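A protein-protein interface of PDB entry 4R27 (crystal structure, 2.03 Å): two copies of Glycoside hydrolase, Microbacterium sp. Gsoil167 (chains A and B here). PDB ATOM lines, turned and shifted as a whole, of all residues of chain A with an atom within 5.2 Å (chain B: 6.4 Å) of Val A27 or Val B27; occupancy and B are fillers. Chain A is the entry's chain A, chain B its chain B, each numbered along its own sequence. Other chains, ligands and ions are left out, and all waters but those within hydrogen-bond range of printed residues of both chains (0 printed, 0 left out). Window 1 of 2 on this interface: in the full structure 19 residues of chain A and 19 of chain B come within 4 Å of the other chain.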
ATOM      1  N   ASN A  25     -22.422  16.263  -8.412  1.00  0.00           N
ATOM      2  CA  ASN A  25     -21.806  15.028  -7.991  1.00  0.00           C
ATOM      3  C   ASN A  25     -21.959  13.916  -9.040  1.00  0.00           C
ATOM      4  O   ASN A  25     -22.301  12.783  -8.730  1.00  0.00           O
ATOM      5  CB  ASN A  25     -22.273  14.675  -6.561  1.00  0.00           C
ATOM      6  CG  ASN A  25     -21.739  15.666  -5.556  1.00  0.00           C
ATOM      7  OD1 ASN A  25     -20.514  15.792  -5.409  1.00  0.00           O
ATOM      8  ND2 ASN A  25     -22.628  16.511  -4.980  1.00  0.00           N
ATOM      9  N   ASN A  26     -21.660  14.228 -10.295  1.00  0.00           N
ATOM     10  CA  ASN A  26     -21.688  13.164 -11.359  1.00  0.00           C
ATOM     11  C   ASN A  26     -20.301  12.521 -11.430  1.00  0.00           C
ATOM     12  O   ASN A  26     -19.648  12.491 -12.521  1.00  0.00           O
ATOM     13  CB  ASN A  26     -22.149  13.710 -12.711  1.00  0.00           C
ATOM     14  CG  ASN A  26     -22.793  12.625 -13.613  1.00  0.00           C
ATOM     15  OD1 ASN A  26     -23.218  11.540 -13.126  1.00  0.00           O
ATOM     16  ND2 ASN A  26     -22.919  12.927 -14.923  1.00  0.00           N
ATOM     17  N   VAL A  27     -19.882  11.984 -10.259  1.00  0.00           N
ATOM     18  CA  VAL A  27     -18.463  11.680  -9.942  1.00  0.00           C
ATOM     19  C   VAL A  27     -17.927  10.479 -10.685  1.00  0.00           C
ATOM     20  O   VAL A  27     -16.674  10.292 -10.850  1.00  0.00           O
ATOM     21  CB  VAL A  27     -18.198  11.543  -8.381  1.00  0.00           C
ATOM     22  CG1 VAL A  27     -18.727  12.752  -7.638  1.00  0.00           C
ATOM     23  CG2 VAL A  27     -18.831  10.278  -7.796  1.00  0.00           C
ATOM     24  N   ASN A  28     -18.847   9.686 -11.215  1.00  0.00           N
ATOM     25  CA  ASN A  28     -18.474   8.499 -11.996  1.00  0.00           C
ATOM     26  C   ASN A  28     -18.417   8.741 -13.516  1.00  0.00           C
ATOM     27  O   ASN A  28     -18.135   7.817 -14.339  1.00  0.00           O
ATOM     28  CB  ASN A  28     -19.415   7.337 -11.674  1.00  0.00           C
ATOM     29  CG  ASN A  28     -18.828   6.012 -12.106  1.00  0.00           C
ATOM     30  OD1 ASN A  28     -17.611   5.760 -11.888  1.00  0.00           O
ATOM     31  ND2 ASN A  28     -19.639   5.184 -12.784  1.00  0.00           N
ATOM     32  N   SER A  29     -18.703   9.976 -13.909  1.00  0.00           N
ATOM     33  CA  SER A  29     -18.741  10.329 -15.304  1.00  0.00           C
ATOM     34  C   SER A  29     -17.333  10.497 -15.907  1.00  0.00           C
ATOM     35  O   SER A  29     -16.395  10.915 -15.233  1.00  0.00           O
ATOM     36  CB  SER A  29     -19.541  11.628 -15.535  1.00  0.00           C
ATOM     37  OG  SER A  29     -18.961  12.751 -14.846  1.00  0.00           O
ATOM     38  N   TRP A  32     -16.492  14.426 -15.488  1.00  0.00           N
ATOM     39  CA  TRP A  32     -15.938  14.701 -14.156  1.00  0.00           C
ATOM     40  C   TRP A  32     -14.459  14.439 -14.118  1.00  0.00           C
ATOM     41  O   TRP A  32     -13.655  15.279 -13.675  1.00  0.00           O
ATOM     42  CB  TRP A  32     -16.607  13.824 -13.081  1.00  0.00           C
ATOM     43  CG  TRP A  32     -16.119  14.111 -11.670  1.00  0.00           C
ATOM     44  CD1 TRP A  32     -14.980  13.637 -11.088  1.00  0.00           C
ATOM     45  CD2 TRP A  32     -16.772  14.907 -10.657  1.00  0.00           C
ATOM     46  NE1 TRP A  32     -14.878  14.099  -9.831  1.00  0.00           N
ATOM     47  CE2 TRP A  32     -15.950  14.883  -9.536  1.00  0.00           C
ATOM     48  CE3 TRP A  32     -17.981  15.630 -10.605  1.00  0.00           C
ATOM     49  CZ2 TRP A  32     -16.259  15.553  -8.368  1.00  0.00           C
ATOM     50  CZ3 TRP A  32     -18.298  16.285  -9.470  1.00  0.00           C
ATOM     51  CH2 TRP A  32     -17.422  16.261  -8.331  1.00  0.00           C
ATOM     52  N   PRO A  82     -22.843   1.887 -12.847  1.00  0.00           N
ATOM     53  CA  PRO A  82     -21.608   2.587 -12.376  1.00  0.00           C
ATOM     54  C   PRO A  82     -20.299   1.828 -12.693  1.00  0.00           C
ATOM     55  O   PRO A  82     -19.223   2.440 -12.732  1.00  0.00           O
ATOM     56  CB  PRO A  82     -21.855   2.762 -10.858  1.00  0.00           C
ATOM     57  CG  PRO A  82     -22.907   1.779 -10.504  1.00  0.00           C
ATOM     58  CD  PRO A  82     -23.747   1.518 -11.737  1.00  0.00           C
ATOM     59  N   HIS B  20     -20.765   2.919   4.041  1.00  0.00           N
ATOM     60  CA  HIS B  20     -20.421   2.051   2.912  1.00  0.00           C
ATOM     61  C   HIS B  20     -21.261   0.770   2.954  1.00  0.00           C
ATOM     62  O   HIS B  20     -21.556   0.202   1.932  1.00  0.00           O
ATOM     63  CB  HIS B  20     -18.932   1.718   2.856  1.00  0.00           C
ATOM     64  CG  HIS B  20     -18.535   1.055   1.574  1.00  0.00           C
ATOM     65  ND1 HIS B  20     -18.409   1.752   0.386  1.00  0.00           N
ATOM     66  CD2 HIS B  20     -18.351  -0.250   1.268  1.00  0.00           C
ATOM     67  CE1 HIS B  20     -18.123   0.903  -0.588  1.00  0.00           C
ATOM     68  NE2 HIS B  20     -18.103  -0.319  -0.081  1.00  0.00           N
ATOM     69  N   GLY B  24     -25.456   2.523  -0.428  1.00  0.00           N
ATOM     70  CA  GLY B  24     -25.482   2.230  -1.839  1.00  0.00           C
ATOM     71  C   GLY B  24     -24.752   3.281  -2.623  1.00  0.00           C
ATOM     72  O   GLY B  24     -24.736   4.431  -2.221  1.00  0.00           O
ATOM     73  N   ASN B  25     -24.127   2.878  -3.717  1.00  0.00           N
ATOM     74  CA  ASN B  25     -23.485   3.795  -4.641  1.00  0.00           C
ATOM     75  C   ASN B  25     -22.473   4.668  -3.956  1.00  0.00           C
ATOM     76  O   ASN B  25     -22.445   5.859  -4.184  1.00  0.00           O
ATOM     77  CB  ASN B  25     -24.463   4.648  -5.411  1.00  0.00           C
ATOM     78  CG  ASN B  25     -25.290   3.802  -6.391  1.00  0.00           C
ATOM     79  OD1 ASN B  25     -24.758   3.100  -7.256  1.00  0.00           O
ATOM     80  ND2 ASN B  25     -26.589   3.793  -6.182  1.00  0.00           N
ATOM     81  N   ASN B  26     -21.555   4.047  -3.203  1.00  0.00           N
ATOM     82  CA  ASN B  26     -20.404   4.806  -2.662  1.00  0.00           C
ATOM     83  C   ASN B  26     -19.223   4.770  -3.609  1.00  0.00           C
ATOM     84  O   ASN B  26     -18.109   4.394  -3.252  1.00  0.00           O
ATOM     85  CB  ASN B  26     -20.083   4.261  -1.273  1.00  0.00           C
ATOM     86  CG  ASN B  26     -19.304   5.240  -0.431  1.00  0.00           C
ATOM     87  OD1 ASN B  26     -19.378   6.465  -0.626  1.00  0.00           O
ATOM     88  ND2 ASN B  26     -18.661   4.725   0.611  1.00  0.00           N
ATOM     89  N   VAL B  27     -19.505   5.180  -4.836  1.00  0.00           N
ATOM     90  CA  VAL B  27     -18.667   4.976  -5.989  1.00  0.00           C
ATOM     91  C   VAL B  27     -17.327   5.713  -5.991  1.00  0.00           C
ATOM     92  O   VAL B  27     -16.451   5.393  -6.780  1.00  0.00           O
ATOM     93  CB  VAL B  27     -19.422   5.354  -7.295  1.00  0.00           C
ATOM     94  CG1 VAL B  27     -20.769   4.600  -7.449  1.00  0.00           C
ATOM     95  CG2 VAL B  27     -19.619   6.857  -7.400  1.00  0.00           C
ATOM     96  N   ASN B  28     -17.185   6.743  -5.163  1.00  0.00           N
ATOM     97  CA  ASN B  28     -15.939   7.462  -5.068  1.00  0.00           C
ATOM     98  C   ASN B  28     -15.040   6.964  -3.973  1.00  0.00           C
ATOM     99  O   ASN B  28     -13.977   7.546  -3.770  1.00  0.00           O
ATOM    100  CB  ASN B  28     -16.181   8.985  -4.852  1.00  0.00           C
ATOM    101  CG  ASN B  28     -14.894   9.825  -5.111  1.00  0.00           C
ATOM    102  OD1 ASN B  28     -14.124   9.570  -6.062  1.00  0.00           O
ATOM    103  ND2 ASN B  28     -14.675  10.828  -4.274  1.00  0.00           N
ATOM    104  N   SER B  29     -15.461   5.944  -3.225  1.00  0.00           N
ATOM    105  CA  SER B  29     -14.659   5.456  -2.087  1.00  0.00           C
ATOM    106  C   SER B  29     -13.567   4.503  -2.485  1.00  0.00           C
ATOM    107  O   SER B  29     -13.664   3.844  -3.531  1.00  0.00           O
ATOM    108  CB  SER B  29     -15.565   4.781  -1.059  1.00  0.00           C
ATOM    109  OG  SER B  29     -16.101   3.532  -1.528  1.00  0.00           O
ATOM    110  N   TRP B  32     -15.071   0.779  -2.715  1.00  0.00           N
ATOM    111  CA  TRP B  32     -15.749   0.555  -3.980  1.00  0.00           C
ATOM    112  C   TRP B  32     -14.714   0.114  -5.022  1.00  0.00           C
ATOM    113  O   TRP B  32     -14.932  -0.911  -5.769  1.00  0.00           O
ATOM    114  CB  TRP B  32     -16.502   1.806  -4.474  1.00  0.00           C
ATOM    115  CG  TRP B  32     -17.124   1.624  -5.782  1.00  0.00           C
ATOM    116  CD1 TRP B  32     -16.504   1.573  -7.006  1.00  0.00           C
ATOM    117  CD2 TRP B  32     -18.506   1.321  -6.020  1.00  0.00           C
ATOM    118  NE1 TRP B  32     -17.448   1.319  -8.014  1.00  0.00           N
ATOM    119  CE2 TRP B  32     -18.674   1.173  -7.420  1.00  0.00           C
ATOM    120  CE3 TRP B  32     -19.646   1.291  -5.189  1.00  0.00           C
ATOM    121  CZ2 TRP B  32     -19.905   0.935  -7.984  1.00  0.00           C
ATOM    122  CZ3 TRP B  32     -20.841   1.034  -5.748  1.00  0.00           C
ATOM    123  CH2 TRP B  32     -20.979   0.894  -7.137  1.00  0.00           C
ATOM    124  N   PHE B  33     -13.602   0.880  -5.077  1.00  0.00           N
ATOM    125  CA  PHE B  33     -12.541   0.652  -6.053  1.00  0.00           C
ATOM    126  C   PHE B  33     -11.944  -0.774  -5.834  1.00  0.00           C
ATOM    127  O   PHE B  33     -11.829  -1.537  -6.781  1.00  0.00           O
ATOM    128  CB  PHE B  33     -11.494   1.753  -5.885  1.00  0.00           C
ATOM    129  CG  PHE B  33     -10.176   1.511  -6.563  1.00  0.00           C
ATOM    130  CD1 PHE B  33     -10.019   1.783  -7.932  1.00  0.00           C
ATOM    131  CD2 PHE B  33      -9.071   1.139  -5.831  1.00  0.00           C
ATOM    132  CE1 PHE B  33      -8.774   1.649  -8.585  1.00  0.00           C
ATOM    133  CE2 PHE B  33      -7.809   0.989  -6.475  1.00  0.00           C
ATOM    134  CZ  PHE B  33      -7.669   1.231  -7.843  1.00  0.00           C
ATOM    135  N   ALA B  78     -15.775  10.270   1.244  1.00  0.00           N
ATOM    136  CA  ALA B  78     -15.798  10.026  -0.177  1.00  0.00           C
ATOM    137  C   ALA B  78     -16.868  10.861  -0.935  1.00  0.00           C
ATOM    138  O   ALA B  78     -16.642  11.312  -2.087  1.00  0.00           O
ATOM    139  CB  ALA B  78     -15.988   8.530  -0.410  1.00  0.00           C
ATOM    140  N   ARG B  79     -18.012  11.117  -0.270  1.00  0.00           N
ATOM    141  CA  ARG B  79     -19.065  11.983  -0.839  1.00  0.00           C
ATOM    142  C   ARG B  79     -18.855  13.486  -0.445  1.00  0.00           C
ATOM    143  O   ARG B  79     -19.256  14.333  -1.184  1.00  0.00           O
ATOM    144  CB  ARG B  79     -20.459  11.558  -0.369  1.00  0.00           C
ATOM    145  CG  ARG B  79     -20.843  10.090  -0.554  1.00  0.00           C
ATOM    146  CD  ARG B  79     -22.247   9.867  -0.005  1.00  0.00           C
ATOM    147  NE  ARG B  79     -22.511   8.444   0.155  1.00  0.00           N
ATOM    148  CZ  ARG B  79     -22.748   7.611  -0.846  1.00  0.00           C
ATOM    149  NH1 ARG B  79     -22.819   8.050  -2.096  1.00  0.00           N
ATOM    150  NH2 ARG B  79     -22.902   6.327  -0.602  1.00  0.00           N
ATOM    151  N   PRO B  82     -15.109  15.023  -2.743  1.00  0.00           N
ATOM    152  CA  PRO B  82     -14.922  13.991  -3.813  1.00  0.00           C
ATOM    153  C   PRO B  82     -13.572  14.113  -4.567  1.00  0.00           C
ATOM    154  O   PRO B  82     -13.079  13.139  -5.154  1.00  0.00           O
ATOM    155  CB  PRO B  82     -16.165  14.177  -4.741  1.00  0.00           C
ATOM    156  CG  PRO B  82     -16.660  15.571  -4.443  1.00  0.00           C
ATOM    157  CD  PRO B  82     -16.251  15.916  -3.030  1.00  0.00           C
ATOM    158  N   GLU B  83     -12.980  15.306  -4.548  1.00  0.00           N
ATOM    159  CA  GLU B  83     -11.608  15.490  -4.996  1.00  0.00           C
ATOM    160  C   GLU B  83     -10.977  16.358  -3.933  1.00  0.00           C
ATOM    161  O   GLU B  83     -11.663  17.129  -3.261  1.00  0.00           O
ATOM    162  CB  GLU B  83     -11.513  16.130  -6.374  1.00  0.00           C
ATOM    163  CG  GLU B  83     -12.255  15.401  -7.464  1.00  0.00           C
ATOM    164  CD  GLU B  83     -11.579  14.129  -7.948  1.00  0.00           C
ATOM    165  OE1 GLU B  83     -10.435  13.850  -7.562  1.00  0.00           O
ATOM    166  OE2 GLU B  83     -12.217  13.384  -8.715  1.00  0.00           O
ATOM    167  N   LEU B 120     -11.270   7.784  -2.785  1.00  0.00           N
ATOM    168  CA  LEU B 120     -10.266   7.053  -3.527  1.00  0.00           C
ATOM    169  C   LEU B 120      -8.969   7.923  -3.652  1.00  0.00           C
ATOM    170  O   LEU B 120      -7.873   7.419  -3.427  1.00  0.00           O
ATOM    171  CB  LEU B 120     -10.765   6.600  -4.907  1.00  0.00           C
ATOM    172  CG  LEU B 120      -9.677   5.942  -5.763  1.00  0.00           C
ATOM    173  CD1 LEU B 120      -9.151   4.676  -5.110  1.00  0.00           C
ATOM    174  CD2 LEU B 120     -10.221   5.669  -7.150  1.00  0.00           C
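The side-chain hydroxyl of Ser B29 sits at hydrogen-bond distance from the backbone NH of Trp B32, 3.2 Å away.
ND2 of Asn B28 lies within hydrogen-bond range of O of Pro B82, at 2.9 Å.
O of Asn B25 sits at hydrogen-bond distance from NH1 of Arg B79 (3.0 Å).
The backbone carbonyl oxygen of Pro A82 lies within hydrogen-bond range of the side-chain amide nitrogen of Asn A28 (2.8 Å).
The backbone NH (N) of Trp A32 lies within hydrogen-bond range of the side-chain hydroxyl (OG) of Ser A29 (3.1 Å).
Of the 14 printed residues of chain B, 5 touch a printed residue of chain A.
Printed residues of chain B that touch a printed residue of chain A: Asn B25, Val B27, Trp B32, Pro B82 and Glu B83.
Along chain B the printed residues that touch a printed residue of chain A span positions 25 to 83.
Of the 7 printed residues of chain A, 4 touch a printed residue of chain B.
Printed residues of chain A that touch a printed residue of chain B: Asn A25, Val A27, Trp A32 and Pro A82.
Among the printed residues, no Asp or Glu carboxylate lies within 4 Å of a Lys or Arg side-chain nitrogen of the other chain.
Asn A25 touches Pro B82, and with the chains exchanged Pro A82 touches Asn B25.
Val B27 touches its own counterpart, Val A27.
Trp A32 touches Pro B82, and with the chains exchanged Pro A82 touches Trp B32.
Val A27 touches just one residue of chain B: Val B27 (3.5 Å).
Printed residues of chain A within 4 Å of Val B27: Val A27.
Printed residues of chain A within 4 Å of Glu B83: Trp A32 (3.0 Å).
Of the printed residues of chain B, Asn A25 touches Pro B82.
Of the printed residues of chain A, Pro B82 touches Asn A25 (3.98 Å) and Trp A32 (3.9 Å).
Of the printed residues of chain B, Pro A82 touches Asn B25 (3.96 Å) and Trp B32 (3.9 Å).
Asn A26 touches none of the printed residues of chain B.
His B20 touches none of the printed residues of chain A.
The nearest residue of chain B that does not touch Val A27 is Pro B82 (4.1 Å).
The nearest printed residue of chain B that does not touch Trp A32 is Asn B28 (5.9 Å).
NE1 of Trp A32 is in hydrogen-bond range of OE2 of Glu B83, at 3.0 Å.
Among the printed residues, merely in contact across the chains: Asn A25 with Pro B82 (3.98 Å), Val A27 with Val B27 (3.5 Å), Trp A32 with Pro B82 (3.9 Å), Pro A82 with Asn B25 (3.96 Å) and Pro A82 with Trp B32 (3.9 Å).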
